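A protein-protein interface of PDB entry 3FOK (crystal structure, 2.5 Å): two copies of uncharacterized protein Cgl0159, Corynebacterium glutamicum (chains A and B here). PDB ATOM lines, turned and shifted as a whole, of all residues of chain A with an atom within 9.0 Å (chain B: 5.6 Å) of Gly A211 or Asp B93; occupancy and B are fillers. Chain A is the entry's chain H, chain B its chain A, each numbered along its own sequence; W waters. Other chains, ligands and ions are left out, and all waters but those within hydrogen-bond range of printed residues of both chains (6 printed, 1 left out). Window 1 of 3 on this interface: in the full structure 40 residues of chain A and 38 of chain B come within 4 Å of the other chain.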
ATOM      1  N   ILE A 151       2.390  33.487   4.288  1.00  0.00           N
ATOM      2  CA  ILE A 151       2.036  34.597   3.422  1.00  0.00           C
ATOM      3  C   ILE A 151       2.699  35.902   3.845  1.00  0.00           C
ATOM      4  O   ILE A 151       2.294  36.529   4.823  1.00  0.00           O
ATOM      5  CB  ILE A 151       0.501  34.773   3.412  1.00  0.00           C
ATOM      6  CG1 ILE A 151      -0.154  33.450   2.997  1.00  0.00           C
ATOM      7  CG2 ILE A 151       0.105  35.905   2.488  1.00  0.00           C
ATOM      8  CD1 ILE A 151      -1.654  33.412   3.147  1.00  0.00           C
ATOM      9  N   LEU A 162       1.732  30.635  -3.272  1.00  0.00           N
ATOM     10  CA  LEU A 162       0.277  30.584  -3.237  1.00  0.00           C
ATOM     11  C   LEU A 162      -0.213  29.733  -4.406  1.00  0.00           C
ATOM     12  O   LEU A 162      -1.074  28.869  -4.242  1.00  0.00           O
ATOM     13  CB  LEU A 162      -0.313  31.990  -3.341  1.00  0.00           C
ATOM     14  CG  LEU A 162      -0.080  32.930  -2.156  1.00  0.00           C
ATOM     15  CD1 LEU A 162      -0.599  34.321  -2.495  1.00  0.00           C
ATOM     16  CD2 LEU A 162      -0.783  32.387  -0.924  1.00  0.00           C
ATOM     17  N   THR A 165       0.629  26.027  -3.982  1.00  0.00           N
ATOM     18  CA  THR A 165      -0.234  25.445  -2.962  1.00  0.00           C
ATOM     19  C   THR A 165      -1.592  25.148  -3.583  1.00  0.00           C
ATOM     20  O   THR A 165      -2.195  24.110  -3.305  1.00  0.00           O
ATOM     21  CB  THR A 165      -0.422  26.399  -1.759  1.00  0.00           C
ATOM     22  OG1 THR A 165       0.830  26.567  -1.082  1.00  0.00           O
ATOM     23  CG2 THR A 165      -1.445  25.834  -0.784  1.00  0.00           C
ATOM     24  N   ALA A 166      -2.068  26.057  -4.429  1.00  0.00           N
ATOM     25  CA  ALA A 166      -3.352  25.871  -5.096  1.00  0.00           C
ATOM     26  C   ALA A 166      -3.293  24.611  -5.948  1.00  0.00           C
ATOM     27  O   ALA A 166      -4.239  23.825  -5.982  1.00  0.00           O
ATOM     28  CB  ALA A 166      -3.676  27.081  -5.969  1.00  0.00           C
ATOM     29  N   VAL A 169      -3.523  21.471  -3.825  1.00  0.00           N
ATOM     30  CA  VAL A 169      -4.890  21.198  -3.413  1.00  0.00           C
ATOM     31  C   VAL A 169      -5.677  20.614  -4.585  1.00  0.00           C
ATOM     32  O   VAL A 169      -6.479  19.701  -4.400  1.00  0.00           O
ATOM     33  CB  VAL A 169      -5.591  22.477  -2.897  1.00  0.00           C
ATOM     34  CG1 VAL A 169      -7.056  22.177  -2.570  1.00  0.00           C
ATOM     35  CG2 VAL A 169      -4.873  22.991  -1.656  1.00  0.00           C
ATOM     36  N   ASN A 170      -5.446  21.139  -5.785  1.00  0.00           N
ATOM     37  CA  ASN A 170      -6.126  20.634  -6.976  1.00  0.00           C
ATOM     38  C   ASN A 170      -5.913  19.127  -7.043  1.00  0.00           C
ATOM     39  O   ASN A 170      -6.865  18.351  -7.135  1.00  0.00           O
ATOM     40  CB  ASN A 170      -5.544  21.249  -8.259  1.00  0.00           C
ATOM     41  CG  ASN A 170      -5.915  22.703  -8.447  1.00  0.00           C
ATOM     42  OD1 ASN A 170      -5.482  23.336  -9.407  1.00  0.00           O
ATOM     43  ND2 ASN A 170      -6.718  23.241  -7.538  1.00  0.00           N
ATOM     44  N   LEU A 181      -3.397  22.367   5.426  1.00  0.00           N
ATOM     45  CA  LEU A 181      -2.652  23.592   5.128  1.00  0.00           C
ATOM     46  C   LEU A 181      -2.317  24.337   6.422  1.00  0.00           C
ATOM     47  O   LEU A 181      -3.193  24.570   7.255  1.00  0.00           O
ATOM     48  CB  LEU A 181      -3.457  24.529   4.216  1.00  0.00           C
ATOM     49  CG  LEU A 181      -3.976  24.040   2.860  1.00  0.00           C
ATOM     50  CD1 LEU A 181      -4.560  25.223   2.107  1.00  0.00           C
ATOM     51  CD2 LEU A 181      -2.857  23.406   2.052  1.00  0.00           C
ATOM     52  N   GLN A 204      -6.919  36.286   8.973  1.00  0.00           N
ATOM     53  CA  GLN A 204      -6.695  36.683   7.591  1.00  0.00           C
ATOM     54  C   GLN A 204      -6.000  35.578   6.802  1.00  0.00           C
ATOM     55  O   GLN A 204      -6.304  35.365   5.626  1.00  0.00           O
ATOM     56  CB  GLN A 204      -5.855  37.957   7.526  1.00  0.00           C
ATOM     57  CG  GLN A 204      -5.817  38.585   6.141  1.00  0.00           C
ATOM     58  CD  GLN A 204      -4.898  39.788   6.063  1.00  0.00           C
ATOM     59  OE1 GLN A 204      -4.845  40.477   5.045  1.00  0.00           O
ATOM     60  NE2 GLN A 204      -4.158  40.042   7.138  1.00  0.00           N
ATOM     61  N   SER A 205      -5.076  34.870   7.445  1.00  0.00           N
ATOM     62  CA  SER A 205      -4.357  33.797   6.769  1.00  0.00           C
ATOM     63  C   SER A 205      -5.279  32.629   6.436  1.00  0.00           C
ATOM     64  O   SER A 205      -5.114  31.970   5.410  1.00  0.00           O
ATOM     65  CB  SER A 205      -3.186  33.299   7.626  1.00  0.00           C
ATOM     66  OG  SER A 205      -3.628  32.615   8.780  1.00  0.00           O
ATOM     67  N   VAL A 206      -6.250  32.376   7.304  1.00  0.00           N
ATOM     68  CA  VAL A 206      -7.185  31.290   7.087  1.00  0.00           C
ATOM     69  C   VAL A 206      -8.100  31.601   5.905  1.00  0.00           C
ATOM     70  O   VAL A 206      -8.350  30.737   5.062  1.00  0.00           O
ATOM     71  CB  VAL A 206      -8.043  31.037   8.343  1.00  0.00           C
ATOM     72  CG1 VAL A 206      -9.099  29.985   8.045  1.00  0.00           C
ATOM     73  CG2 VAL A 206      -7.160  30.573   9.484  1.00  0.00           C
ATOM     74  N   ALA A 207      -8.592  32.835   5.845  1.00  0.00           N
ATOM     75  CA  ALA A 207      -9.476  33.246   4.762  1.00  0.00           C
ATOM     76  C   ALA A 207      -8.773  33.101   3.416  1.00  0.00           C
ATOM     77  O   ALA A 207      -9.405  32.781   2.408  1.00  0.00           O
ATOM     78  CB  ALA A 207      -9.923  34.688   4.970  1.00  0.00           C
ATOM     79  N   ILE A 208      -7.464  33.340   3.404  1.00  0.00           N
ATOM     80  CA  ILE A 208      -6.683  33.231   2.178  1.00  0.00           C
ATOM     81  C   ILE A 208      -6.410  31.772   1.825  1.00  0.00           C
ATOM     82  O   ILE A 208      -6.664  31.345   0.701  1.00  0.00           O
ATOM     83  CB  ILE A 208      -5.338  33.980   2.312  1.00  0.00           C
ATOM     84  CG1 ILE A 208      -5.597  35.486   2.418  1.00  0.00           C
ATOM     85  CG2 ILE A 208      -4.437  33.668   1.120  1.00  0.00           C
ATOM     86  CD1 ILE A 208      -4.362  36.303   2.751  1.00  0.00           C
ATOM     87  N   ALA A 209      -5.904  31.009   2.787  1.00  0.00           N
ATOM     88  CA  ALA A 209      -5.599  29.602   2.555  1.00  0.00           C
ATOM     89  C   ALA A 209      -6.826  28.808   2.119  1.00  0.00           C
ATOM     90  O   ALA A 209      -6.754  28.006   1.186  1.00  0.00           O
ATOM     91  CB  ALA A 209      -4.997  28.983   3.814  1.00  0.00           C
ATOM     92  N   ALA A 210      -7.949  29.033   2.794  1.00  0.00           N
ATOM     93  CA  ALA A 210      -9.184  28.330   2.481  1.00  0.00           C
ATOM     94  C   ALA A 210      -9.579  28.486   1.021  1.00  0.00           C
ATOM     95  O   ALA A 210     -10.185  27.590   0.437  1.00  0.00           O
ATOM     96  CB  ALA A 210     -10.309  28.833   3.380  1.00  0.00           C
ATOM     97  N   GLY A 211      -9.234  29.625   0.432  1.00  0.00           N
ATOM     98  CA  GLY A 211      -9.590  29.874  -0.954  1.00  0.00           C
ATOM     99  C   GLY A 211      -8.643  29.303  -1.993  1.00  0.00           C
ATOM    100  O   GLY A 211      -8.860  29.498  -3.192  1.00  0.00           O
ATOM    101  N   LEU A 212      -7.600  28.602  -1.550  1.00  0.00           N
ATOM    102  CA  LEU A 212      -6.627  28.016  -2.470  1.00  0.00           C
ATOM    103  C   LEU A 212      -7.072  26.642  -2.955  1.00  0.00           C
ATOM    104  O   LEU A 212      -7.413  25.775  -2.148  1.00  0.00           O
ATOM    105  CB  LEU A 212      -5.261  27.894  -1.789  1.00  0.00           C
ATOM    106  CG  LEU A 212      -4.597  29.188  -1.310  1.00  0.00           C
ATOM    107  CD1 LEU A 212      -3.309  28.853  -0.568  1.00  0.00           C
ATOM    108  CD2 LEU A 212      -4.318  30.094  -2.494  1.00  0.00           C
ATOM    109  N   GLY A 213      -7.056  26.441  -4.270  1.00  0.00           N
ATOM    110  CA  GLY A 213      -7.469  25.166  -4.826  1.00  0.00           C
ATOM    111  C   GLY A 213      -8.743  25.332  -5.630  1.00  0.00           C
ATOM    112  O   GLY A 213      -9.459  26.317  -5.453  1.00  0.00           O
ATOM    113  N   ASN A 214      -9.030  24.381  -6.514  1.00  0.00           N
ATOM    114  CA  ASN A 214     -10.232  24.454  -7.342  1.00  0.00           C
ATOM    115  C   ASN A 214     -11.344  23.584  -6.769  1.00  0.00           C
ATOM    116  O   ASN A 214     -12.390  23.397  -7.387  1.00  0.00           O
ATOM    117  CB  ASN A 214      -9.919  24.019  -8.778  1.00  0.00           C
ATOM    118  CG  ASN A 214      -9.506  22.562  -8.877  1.00  0.00           C
ATOM    119  OD1 ASN A 214      -9.243  22.059  -9.974  1.00  0.00           O
ATOM    120  ND2 ASN A 214      -9.447  21.875  -7.738  1.00  0.00           N
ATOM    121  N   ASP A 215     -11.090  23.057  -5.580  1.00  0.00           N
ATOM    122  CA  ASP A 215     -12.022  22.195  -4.869  1.00  0.00           C
ATOM    123  C   ASP A 215     -11.509  22.171  -3.439  1.00  0.00           C
ATOM    124  O   ASP A 215     -10.450  21.611  -3.171  1.00  0.00           O
ATOM    125  CB  ASP A 215     -11.978  20.780  -5.459  1.00  0.00           C
ATOM    126  CG  ASP A 215     -12.918  19.815  -4.757  1.00  0.00           C
ATOM    127  OD1 ASP A 215     -13.385  20.127  -3.640  1.00  0.00           O
ATOM    128  OD2 ASP A 215     -13.182  18.733  -5.322  1.00  0.00           O
ATOM    129  N   SER A 216     -12.230  22.794  -2.518  1.00  0.00           N
ATOM    130  CA  SER A 216     -11.775  22.794  -1.136  1.00  0.00           C
ATOM    131  C   SER A 216     -12.686  21.958  -0.260  1.00  0.00           C
ATOM    132  O   SER A 216     -13.220  22.439   0.736  1.00  0.00           O
ATOM    133  CB  SER A 216     -11.678  24.226  -0.599  1.00  0.00           C
ATOM    134  OG  SER A 216     -10.322  24.560  -0.293  1.00  0.00           O
ATOM    135  N   SER A 217     -12.865  20.698  -0.647  1.00  0.00           N
ATOM    136  CA  SER A 217     -13.715  19.783   0.101  1.00  0.00           C
ATOM    137  C   SER A 217     -12.871  18.750   0.840  1.00  0.00           C
ATOM    138  O   SER A 217     -13.394  17.924   1.583  1.00  0.00           O
ATOM    139  CB  SER A 217     -14.701  19.078  -0.840  1.00  0.00           C
ATOM    140  OG  SER A 217     -14.032  18.225  -1.755  1.00  0.00           O
ATOM    141  N   TYR A 218     -11.561  18.799   0.627  1.00  0.00           N
ATOM    142  CA  TYR A 218     -10.648  17.882   1.288  1.00  0.00           C
ATOM    143  C   TYR A 218      -9.564  18.623   2.047  1.00  0.00           C
ATOM    144  O   TYR A 218      -8.579  18.020   2.470  1.00  0.00           O
ATOM    145  CB  TYR A 218      -9.986  16.953   0.276  1.00  0.00           C
ATOM    146  CG  TYR A 218     -10.834  15.766  -0.089  1.00  0.00           C
ATOM    147  CD1 TYR A 218     -11.825  15.869  -1.060  1.00  0.00           C
ATOM    148  CD2 TYR A 218     -10.694  14.556   0.589  1.00  0.00           C
ATOM    149  CE1 TYR A 218     -12.662  14.797  -1.347  1.00  0.00           C
ATOM    150  CE2 TYR A 218     -11.523  13.481   0.315  1.00  0.00           C
ATOM    151  CZ  TYR A 218     -12.509  13.607  -0.652  1.00  0.00           C
ATOM    152  OH  TYR A 218     -13.348  12.548  -0.907  1.00  0.00           O
ATOM    153  N   THR A 219      -9.739  19.922   2.246  1.00  0.00           N
ATOM    154  CA  THR A 219      -8.710  20.674   2.934  1.00  0.00           C
ATOM    155  C   THR A 219      -8.981  20.934   4.410  1.00  0.00           C
ATOM    156  O   THR A 219     -10.086  21.306   4.808  1.00  0.00           O
ATOM    157  CB  THR A 219      -8.420  22.014   2.205  1.00  0.00           C
ATOM    158  OG1 THR A 219      -9.115  23.083   2.850  1.00  0.00           O
ATOM    159  CG2 THR A 219      -8.860  21.939   0.754  1.00  0.00           C
ATOM    160  N   MET A 221      -7.183  22.583   8.202  1.00  0.00           N
ATOM    161  CA  MET A 221      -6.362  23.698   8.653  1.00  0.00           C
ATOM    162  C   MET A 221      -5.513  23.230   9.824  1.00  0.00           C
ATOM    163  O   MET A 221      -5.957  22.446  10.659  1.00  0.00           O
ATOM    164  CB  MET A 221      -7.232  24.869   9.111  1.00  0.00           C
ATOM    165  CG  MET A 221      -8.025  25.562   8.007  1.00  0.00           C
ATOM    166  SD  MET A 221      -6.952  26.718   6.882  1.00  0.00           S
ATOM    167  CE  MET A 221      -6.928  25.658   5.278  1.00  0.00           C
ATOM    168  N   SER A 235     -13.577  31.634  11.668  1.00  0.00           N
ATOM    169  CA  SER A 235     -12.991  31.932  10.362  1.00  0.00           C
ATOM    170  C   SER A 235     -13.304  30.875   9.310  1.00  0.00           C
ATOM    171  O   SER A 235     -13.424  31.194   8.129  1.00  0.00           O
ATOM    172  CB  SER A 235     -11.473  32.077  10.473  1.00  0.00           C
ATOM    173  OG  SER A 235     -11.114  33.275  11.137  1.00  0.00           O
ATOM    174  N   THR A 236     -13.415  29.619   9.734  1.00  0.00           N
ATOM    175  CA  THR A 236     -13.725  28.540   8.804  1.00  0.00           C
ATOM    176  C   THR A 236     -14.674  27.508   9.354  1.00  0.00           C
ATOM    177  O   THR A 236     -14.967  27.461  10.544  1.00  0.00           O
ATOM    178  CB  THR A 236     -12.475  27.760   8.342  1.00  0.00           C
ATOM    179  OG1 THR A 236     -11.609  27.537   9.458  1.00  0.00           O
ATOM    180  CG2 THR A 236     -11.751  28.504   7.239  1.00  0.00           C
ATOM    181  N   THR A 237     -15.129  26.667   8.442  1.00  0.00           N
ATOM    182  CA  THR A 237     -16.038  25.581   8.738  1.00  0.00           C
ATOM    183  C   THR A 237     -15.243  24.299   8.540  1.00  0.00           C
ATOM    184  O   THR A 237     -15.767  23.195   8.689  1.00  0.00           O
ATOM    185  CB  THR A 237     -17.208  25.587   7.752  1.00  0.00           C
ATOM    186  OG1 THR A 237     -16.694  25.590   6.416  1.00  0.00           O
ATOM    187  CG2 THR A 237     -18.069  26.821   7.954  1.00  0.00           C
ATOM    188  N   MET A 238     -13.965  24.462   8.218  1.00  0.00           N
ATOM    189  CA  MET A 238     -13.093  23.330   7.959  1.00  0.00           C
ATOM    190  C   MET A 238     -12.485  22.654   9.172  1.00  0.00           C
ATOM    191  O   MET A 238     -12.211  23.293  10.189  1.00  0.00           O
ATOM    192  CB  MET A 238     -11.985  23.761   7.008  1.00  0.00           C
ATOM    193  CG  MET A 238     -12.530  24.284   5.698  1.00  0.00           C
ATOM    194  SD  MET A 238     -11.196  25.070   4.594  1.00  0.00           S
ATOM    195  CE  MET A 238     -12.028  24.752   2.876  1.00  0.00           C
ATOM    196  N   ARG B  18     -17.560  17.850   6.136  1.00  0.00           N
ATOM    197  CA  ARG B  18     -16.223  18.074   5.599  1.00  0.00           C
ATOM    198  C   ARG B  18     -15.199  17.161   6.262  1.00  0.00           C
ATOM    199  O   ARG B  18     -14.255  16.692   5.620  1.00  0.00           O
ATOM    200  CB  ARG B  18     -15.801  19.526   5.819  1.00  0.00           C
ATOM    201  CG  ARG B  18     -16.445  20.538   4.886  1.00  0.00           C
ATOM    202  CD  ARG B  18     -16.041  21.952   5.288  1.00  0.00           C
ATOM    203  NE  ARG B  18     -16.053  22.872   4.158  1.00  0.00           N
ATOM    204  CZ  ARG B  18     -15.196  22.819   3.143  1.00  0.00           C
ATOM    205  NH1 ARG B  18     -14.252  21.885   3.116  1.00  0.00           N
ATOM    206  NH2 ARG B  18     -15.282  23.701   2.154  1.00  0.00           N
ATOM    207  N   ALA B  53     -10.873  35.376   0.251  1.00  0.00           N
ATOM    208  CA  ALA B  53      -9.779  34.621  -0.353  1.00  0.00           C
ATOM    209  C   ALA B  53      -8.670  35.509  -0.910  1.00  0.00           C
ATOM    210  O   ALA B  53      -7.554  35.051  -1.133  1.00  0.00           O
ATOM    211  CB  ALA B  53     -10.325  33.723  -1.453  1.00  0.00           C
ATOM    212  N   ARG B  69     -16.711  33.634   9.035  1.00  0.00           N
ATOM    213  CA  ARG B  69     -17.261  32.848   7.943  1.00  0.00           C
ATOM    214  C   ARG B  69     -18.691  32.368   8.185  1.00  0.00           C
ATOM    215  O   ARG B  69     -19.477  32.251   7.239  1.00  0.00           O
ATOM    216  CB  ARG B  69     -16.342  31.656   7.650  1.00  0.00           C
ATOM    217  CG  ARG B  69     -16.809  30.766   6.504  1.00  0.00           C
ATOM    218  CD  ARG B  69     -16.897  31.515   5.168  1.00  0.00           C
ATOM    219  NE  ARG B  69     -15.687  31.392   4.352  1.00  0.00           N
ATOM    220  CZ  ARG B  69     -14.740  32.321   4.260  1.00  0.00           C
ATOM    221  NH1 ARG B  69     -14.847  33.460   4.936  1.00  0.00           N
ATOM    222  NH2 ARG B  69     -13.687  32.117   3.476  1.00  0.00           N
ATOM    223  N   THR B  91     -15.419  31.746  -4.185  1.00  0.00           N
ATOM    224  CA  THR B  91     -14.248  30.907  -4.341  1.00  0.00           C
ATOM    225  C   THR B  91     -14.731  29.496  -3.984  1.00  0.00           C
ATOM    226  O   THR B  91     -15.807  29.340  -3.406  1.00  0.00           O
ATOM    227  CB  THR B  91     -13.118  31.392  -3.401  1.00  0.00           C
ATOM    228  OG1 THR B  91     -12.412  30.271  -2.866  1.00  0.00           O
ATOM    229  CG2 THR B  91     -13.691  32.223  -2.269  1.00  0.00           C
ATOM    230  N   PRO B  92     -13.962  28.452  -4.325  1.00  0.00           N
ATOM    231  CA  PRO B  92     -14.402  27.087  -4.007  1.00  0.00           C
ATOM    232  C   PRO B  92     -14.828  26.797  -2.560  1.00  0.00           C
ATOM    233  O   PRO B  92     -15.767  26.033  -2.334  1.00  0.00           O
ATOM    234  CB  PRO B  92     -13.212  26.230  -4.433  1.00  0.00           C
ATOM    235  CG  PRO B  92     -12.647  27.004  -5.582  1.00  0.00           C
ATOM    236  CD  PRO B  92     -12.686  28.431  -5.064  1.00  0.00           C
ATOM    237  N   ASP B  93     -14.146  27.381  -1.579  1.00  0.00           N
ATOM    238  CA  ASP B  93     -14.491  27.126  -0.178  1.00  0.00           C
ATOM    239  C   ASP B  93     -15.861  27.682   0.218  1.00  0.00           C
ATOM    240  O   ASP B  93     -16.540  27.123   1.080  1.00  0.00           O
ATOM    241  CB  ASP B  93     -13.418  27.701   0.745  1.00  0.00           C
ATOM    242  CG  ASP B  93     -13.338  29.213   0.667  1.00  0.00           C
ATOM    243  OD1 ASP B  93     -13.027  29.741  -0.426  1.00  0.00           O
ATOM    244  OD2 ASP B  93     -13.590  29.873   1.701  1.00  0.00           O
ATOM    245  N   ILE B  94     -16.260  28.783  -0.413  1.00  0.00           N
ATOM    246  CA  ILE B  94     -17.551  29.408  -0.141  1.00  0.00           C
ATOM    247  C   ILE B  94     -18.669  28.632  -0.837  1.00  0.00           C
ATOM    248  O   ILE B  94     -19.717  28.365  -0.247  1.00  0.00           O
ATOM    249  CB  ILE B  94     -17.577  30.882  -0.641  1.00  0.00           C
ATOM    250  CG1 ILE B  94     -16.593  31.731   0.174  1.00  0.00           C
ATOM    251  CG2 ILE B  94     -18.988  31.461  -0.522  1.00  0.00           C
ATOM    252  CD1 ILE B  94     -17.014  31.963   1.615  1.00  0.00           C
ATOM    253  N   ILE B  95     -18.434  28.265  -2.092  1.00  0.00           N
ATOM    254  CA  ILE B  95     -19.434  27.531  -2.850  1.00  0.00           C
ATOM    255  C   ILE B  95     -19.687  26.134  -2.288  1.00  0.00           C
ATOM    256  O   ILE B  95     -20.838  25.709  -2.191  1.00  0.00           O
ATOM    257  CB  ILE B  95     -19.045  27.437  -4.340  1.00  0.00           C
ATOM    258  CG1 ILE B  95     -18.977  28.842  -4.937  1.00  0.00           C
ATOM    259  CG2 ILE B  95     -20.057  26.597  -5.099  1.00  0.00           C
ATOM    260  CD1 ILE B  95     -20.247  29.662  -4.750  1.00  0.00           C
ATOM    261  N   ASP B  96     -18.629  25.422  -1.908  1.00  0.00           N
ATOM    262  CA  ASP B  96     -18.814  24.086  -1.356  1.00  0.00           C
ATOM    263  C   ASP B  96     -19.699  24.132  -0.108  1.00  0.00           C
ATOM    264  O   ASP B  96     -20.628  23.334   0.012  1.00  0.00           O
ATOM    265  CB  ASP B  96     -17.469  23.422  -1.029  1.00  0.00           C
ATOM    266  CG  ASP B  96     -16.635  23.131  -2.277  1.00  0.00           C
ATOM    267  OD1 ASP B  96     -17.222  22.881  -3.354  1.00  0.00           O
ATOM    268  OD2 ASP B  96     -15.388  23.136  -2.181  1.00  0.00           O
ATOM    269  N   ASP B  97     -19.432  25.056   0.814  1.00  0.00           N
ATOM    270  CA  ASP B  97     -20.264  25.139   2.010  1.00  0.00           C
ATOM    271  C   ASP B  97     -21.720  25.339   1.599  1.00  0.00           C
ATOM    272  O   ASP B  97     -22.581  24.530   1.940  1.00  0.00           O
ATOM    273  CB  ASP B  97     -19.821  26.283   2.925  1.00  0.00           C
ATOM    274  CG  ASP B  97     -18.495  26.002   3.612  1.00  0.00           C
ATOM    275  OD1 ASP B  97     -18.184  24.813   3.845  1.00  0.00           O
ATOM    276  OD2 ASP B  97     -17.770  26.971   3.933  1.00  0.00           O
ATOM    277  N   LEU B  98     -21.989  26.408   0.855  1.00  0.00           N
ATOM    278  CA  LEU B  98     -23.345  26.688   0.400  1.00  0.00           C
ATOM    279  C   LEU B  98     -23.953  25.481  -0.311  1.00  0.00           C
ATOM    280  O   LEU B  98     -25.145  25.215  -0.183  1.00  0.00           O
ATOM    281  CB  LEU B  98     -23.356  27.896  -0.539  1.00  0.00           C
ATOM    282  CG  LEU B  98     -23.093  29.280   0.061  1.00  0.00           C
ATOM    283  CD1 LEU B  98     -22.977  30.315  -1.052  1.00  0.00           C
ATOM    284  CD2 LEU B  98     -24.221  29.645   1.019  1.00  0.00           C
ATOM    285  N   THR B 130      -5.336  31.095  -8.479  1.00  0.00           N
ATOM    286  CA  THR B 130      -5.300  30.248  -7.294  1.00  0.00           C
ATOM    287  C   THR B 130      -6.596  29.552  -6.887  1.00  0.00           C
ATOM    288  O   THR B 130      -6.595  28.772  -5.931  1.00  0.00           O
ATOM    289  CB  THR B 130      -4.849  31.084  -6.084  1.00  0.00           C
ATOM    290  OG1 THR B 130      -5.773  32.165  -5.896  1.00  0.00           O
ATOM    291  CG2 THR B 130      -3.463  31.666  -6.322  1.00  0.00           C
ATOM    292  N   GLY B 131      -7.697  29.826  -7.583  1.00  0.00           N
ATOM    293  CA  GLY B 131      -8.955  29.204  -7.206  1.00  0.00           C
ATOM    294  C   GLY B 131      -9.514  28.223  -8.216  1.00  0.00           C
ATOM    295  O   GLY B 131      -8.859  27.244  -8.580  1.00  0.00           O
HETATM  296  O   HOH W   1     -11.961  32.535   1.443  1.00  0.00           O
HETATM  297  O   HOH W   2      -7.658  31.727  -4.131  1.00  0.00           O
HETATM  298  O   HOH W   3     -12.158  17.460   4.172  1.00  0.00           O
HETATM  299  O   HOH W   4      -6.217  26.430  -8.593  1.00  0.00           O
HETATM  300  O   HOH W   5      -6.688  32.359  -1.776  1.00  0.00           O
HETATM  301  O   HOH W   6     -12.632  20.264   4.527  1.00  0.00           O
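The side-chain carboxylate of Asp B93 lies within salt-bridge range of the guanidinium group of Arg B69 (2.9 Å).
OG1 of Thr B91 sits at hydrogen-bond distance from OD1 of Asp B93, at 2.6 Å.
The backbone carbonyl oxygen (O) of Ala A166 lies within hydrogen-bond range of the side-chain amide nitrogen (ND2) of Asn A170, at 3.0 Å.
The side-chain amide nitrogen (ND2) of Asn A170 lies close to the backbone NH (N) of Asn A214 (2.8 Å).
OG of Ser A216 sits at hydrogen-bond distance from O of Ala A210 (3.1 Å).
OD1 of Asp A215 lies within hydrogen-bond range of OG of Ser A217 (2.8 Å).
Water W2 lies within hydrogen-bond range of the side-chain hydroxyl of Thr B130 (2.6 Å) and the backbone carbonyl oxygen of Gly A211 (2.7 Å).
Water W3 lies within hydrogen-bond range of the backbone carbonyl oxygen (O) of Arg B18 and the backbone carbonyl oxygen (O) of Ser A217.
Water W6 bridges the guanidinium group of Arg B18 (2.7 Å) and the backbone carbonyl oxygen of Thr A219 (2.8 Å).
Water W1 lies within hydrogen-bond range of NH2 of Arg B69 (2.7 Å), O of Ala A207 (2.7 Å), OD2 of Asp B93 (3.1 Å) and N of Ala B53 (3.3 Å).
The guanidinium group (NH1) of Arg B18 sits at hydrogen-bond distance from the backbone carbonyl oxygen (O) of Ser A216.
The backbone NH (N) of Ser A216 sits at hydrogen-bond distance from the side-chain carboxylate (OD2) of Asp B96 (3.2 Å).
The side-chain carboxylate (OD2) of Asp B97 lies within hydrogen-bond range of the side-chain hydroxyl (OG1) of Thr A237, at 3.0 Å.
The backbone NH (N) of Gly A213 lies within hydrogen-bond range of the backbone carbonyl oxygen (O) of Thr B130 (2.9 Å).
O of Gly A213 lies close to O of Gly B131, at 3.3 Å.
Among the printed residues, pairs that only touch across the chains: Ala A166 with Thr B130 (3.4 Å), Ala A207 with Ala B53 (3.3 Å), Ile A208 with Ala B53 (3.9 Å), Ala A210 with Asp B93 (3.2 Å), Gly A211 with Ala B53 (3.95 Å), Gly A211 with Thr B91 (3.4 Å), Gly A211 with Asp B93 (3.5 Å), Gly A211 with Thr B130 (3.6 Å), Leu A212 with Thr B130 (3.5 Å), Gly A213 with Pro B92 (3.3 Å), Asn A214 with Pro B92 (3.8 Å), Asn A214 with Gly B131 (3.3 Å), Asp A215 with Pro B92 (3.99 Å), Asp A215 with Asp B96 (3.9 Å), Ser A217 with Arg B18 (3.7 Å), Ser A217 with Asp B96 (3.8 Å), Ser A235 with Arg B69 (3.0 Å), Thr A237 with Arg B18 (3.6 Å), Met A238 with Arg B18 (3.5 Å) and Met A238 with Asp B93 (3.9 Å).
No position is printed for both chains.
Of the 25 pairs that touch across the chains among the printed residues, none has its exchanged pair printed and touching as well.
Of the 13 printed residues of chain B, 10 touch a printed residue of chain A.
Of the 28 printed residues of chain A, 14 touch a printed residue of chain B.
Printed residues of chain A that touch a printed residue of chain B: Ala A166, Ala A207, Ile A208, Ala A210, Gly A211, Leu A212, Gly A213, Asn A214, Asp A215, Ser A216, Ser A217, Ser A235, Thr A237 and Met A238.
Ile A151 touches none of the printed residues of chain B.
Of the printed residues of chain B, Ala A166 touches Thr B130.
Of chain B, only Ala B53 (3.95 Å), Thr B91 (3.4 Å), Asp B93 (3.5 Å) and Thr B130 (3.6 Å) come within 4 Å of Gly A211.
Thr B91 touches just one residue of chain A: Gly A211.
Asp B93 touches just these residues of chain A: Ala A210, Gly A211 and Met A238.
Ile B95 touches none of the printed residues of chain A.
Printed residues of chain A within 4 Å of Thr B130: Ala A166 (3.4 Å), Gly A211 (3.6 Å), Leu A212 (3.5 Å) and Gly A213 (2.9 Å).
The nearest residue of chain B that does not touch Gly A211 is Gly B131 (4.03 Å).
The nearest residue of chain A that does not touch Asp B93 is Ser A216 (4.1 Å).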
